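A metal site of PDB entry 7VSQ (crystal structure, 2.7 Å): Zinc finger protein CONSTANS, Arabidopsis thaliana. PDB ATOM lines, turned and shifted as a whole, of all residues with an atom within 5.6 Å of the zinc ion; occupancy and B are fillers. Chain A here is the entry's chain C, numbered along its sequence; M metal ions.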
ATOM      1  N   CYS A  67     -21.650  20.269  19.274  1.00  0.00           N
ATOM      2  CA  CYS A  67     -22.980  20.128  19.845  1.00  0.00           C
ATOM      3  C   CYS A  67     -24.032  20.242  18.775  1.00  0.00           C
ATOM      4  O   CYS A  67     -23.922  21.093  17.904  1.00  0.00           O
ATOM      5  CB  CYS A  67     -23.242  21.181  20.919  1.00  0.00           C
ATOM      6  SG  CYS A  67     -24.874  20.978  21.707  1.00  0.00           S
ATOM      7  N   GLU A  68     -25.060  19.398  18.833  1.00  0.00           N
ATOM      8  CA  GLU A  68     -26.182  19.498  17.902  1.00  0.00           C
ATOM      9  C   GLU A  68     -27.180  20.533  18.351  1.00  0.00           C
ATOM     10  O   GLU A  68     -27.796  21.190  17.525  1.00  0.00           O
ATOM     11  CB  GLU A  68     -26.860  18.168  17.792  1.00  0.00           C
ATOM     12  CG  GLU A  68     -26.209  17.249  16.812  1.00  0.00           C
ATOM     13  CD  GLU A  68     -26.739  15.884  17.054  1.00  0.00           C
ATOM     14  OE1 GLU A  68     -26.816  15.657  18.260  1.00  0.00           O
ATOM     15  OE2 GLU A  68     -27.038  15.111  16.128  1.00  0.00           O
ATOM     16  N   ALA A  69     -27.362  20.656  19.661  1.00  0.00           N
ATOM     17  CA  ALA A  69     -28.379  21.558  20.168  1.00  0.00           C
ATOM     18  C   ALA A  69     -27.992  23.016  19.966  1.00  0.00           C
ATOM     19  O   ALA A  69     -28.795  23.817  19.486  1.00  0.00           O
ATOM     20  CB  ALA A  69     -28.670  21.264  21.633  1.00  0.00           C
ATOM     21  N   ASP A  70     -26.758  23.366  20.317  1.00  0.00           N
ATOM     22  CA  ASP A  70     -26.295  24.747  20.165  1.00  0.00           C
ATOM     23  C   ASP A  70     -25.744  25.046  18.774  1.00  0.00           C
ATOM     24  O   ASP A  70     -25.528  26.203  18.425  1.00  0.00           O
ATOM     25  CB  ASP A  70     -25.233  25.069  21.205  1.00  0.00           C
ATOM     26  CG  ASP A  70     -25.780  25.076  22.621  1.00  0.00           C
ATOM     27  OD1 ASP A  70     -26.604  25.951  22.939  1.00  0.00           O
ATOM     28  OD2 ASP A  70     -25.375  24.213  23.428  1.00  0.00           O
ATOM     29  N   VAL A  82     -20.641  27.331  28.561  1.00  0.00           N
ATOM     30  CA  VAL A  82     -21.984  27.412  27.991  1.00  0.00           C
ATOM     31  C   VAL A  82     -22.928  26.495  28.723  1.00  0.00           C
ATOM     32  O   VAL A  82     -24.084  26.805  28.912  1.00  0.00           O
ATOM     33  CB  VAL A  82     -21.987  27.004  26.531  1.00  0.00           C
ATOM     34  CG1 VAL A  82     -23.399  26.943  25.957  1.00  0.00           C
ATOM     35  CG2 VAL A  82     -21.179  27.987  25.731  1.00  0.00           C
ATOM     36  N   HIS A  83     -22.435  25.336  29.070  1.00  0.00           N
ATOM     37  CA  HIS A  83     -23.286  24.342  29.703  1.00  0.00           C
ATOM     38  C   HIS A  83     -23.169  24.337  31.231  1.00  0.00           C
ATOM     39  O   HIS A  83     -23.698  23.457  31.901  1.00  0.00           O
ATOM     40  CB  HIS A  83     -22.998  22.971  29.103  1.00  0.00           C
ATOM     41  CG  HIS A  83     -23.096  22.945  27.612  1.00  0.00           C
ATOM     42  ND1 HIS A  83     -22.117  23.455  26.781  1.00  0.00           N
ATOM     43  CD2 HIS A  83     -24.094  22.513  26.788  1.00  0.00           C
ATOM     44  CE1 HIS A  83     -22.488  23.310  25.518  1.00  0.00           C
ATOM     45  NE2 HIS A  83     -23.686  22.740  25.500  1.00  0.00           N
ATOM     46  N   ALA A  89     -28.956  23.317  29.747  1.00  0.00           N
ATOM     47  CA  ALA A  89     -27.724  23.291  28.983  1.00  0.00           C
ATOM     48  C   ALA A  89     -26.912  22.015  29.187  1.00  0.00           C
ATOM     49  O   ALA A  89     -26.378  21.473  28.234  1.00  0.00           O
ATOM     50  CB  ALA A  89     -26.865  24.497  29.328  1.00  0.00           C
ATOM     51  N   HIS A  92     -27.743  18.817  27.241  1.00  0.00           N
ATOM     52  CA  HIS A  92     -27.161  18.719  25.916  1.00  0.00           C
ATOM     53  C   HIS A  92     -26.151  17.592  25.875  1.00  0.00           C
ATOM     54  O   HIS A  92     -25.278  17.509  26.745  1.00  0.00           O
ATOM     55  CB  HIS A  92     -26.445  20.015  25.518  1.00  0.00           C
ATOM     56  CG  HIS A  92     -27.366  21.160  25.250  1.00  0.00           C
ATOM     57  ND1 HIS A  92     -26.908  22.385  24.825  1.00  0.00           N
ATOM     58  CD2 HIS A  92     -28.709  21.271  25.372  1.00  0.00           C
ATOM     59  CE1 HIS A  92     -27.929  23.201  24.677  1.00  0.00           C
ATOM     60  NE2 HIS A  92     -29.034  22.550  25.000  1.00  0.00           N
ATOM     61  N   ARG A  94     -23.112  16.535  24.049  1.00  0.00           N
ATOM     62  CA  ARG A  94     -22.136  17.067  23.139  1.00  0.00           C
ATOM     63  C   ARG A  94     -21.154  15.941  22.883  1.00  0.00           C
ATOM     64  O   ARG A  94     -21.011  15.018  23.692  1.00  0.00           O
ATOM     65  CB  ARG A  94     -21.504  18.317  23.747  1.00  0.00           C
ATOM     66  CG  ARG A  94     -21.730  18.316  25.252  1.00  0.00           C
ATOM     67  CD  ARG A  94     -21.441  19.633  25.956  1.00  0.00           C
ATOM     68  NE  ARG A  94     -21.739  19.488  27.374  1.00  0.00           N
ATOM     69  CZ  ARG A  94     -21.228  20.237  28.357  1.00  0.00           C
ATOM     70  NH1 ARG A  94     -20.377  21.210  28.084  1.00  0.00           N
ATOM     71  NH2 ARG A  94     -21.579  20.015  29.603  1.00  0.00           N
HETATM   72 ZN    ZN M   1     -25.024  22.218  23.551  1.00  0.00          ZN
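SG of Cys 67 sits close to N of Ala 69, at 3.2 Å.
A ring nitrogen (ND1) of His 83 lies within hydrogen-bond range of the guanidinium group of Arg 94 (3.1 Å).
Of the 9 residues printed, 4 come within 4 Å of the zinc ion.
The nearest printed residue that does not touch the zinc ion is Ala 69 (4.2 Å).
OD2 of Asp 70 binds the zinc ion (2.0 Å).
The side-chain sulfur (SG) of Cys 67 binds the zinc ion (2.2 Å).
ND1 of His 92 is bound to the zinc ion, at 2.3 Å.
A ring nitrogen (NE2) of His 83 is bound to the zinc ion, 2.4 Å away.
The zinc ion has four donor atoms within binding distance.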
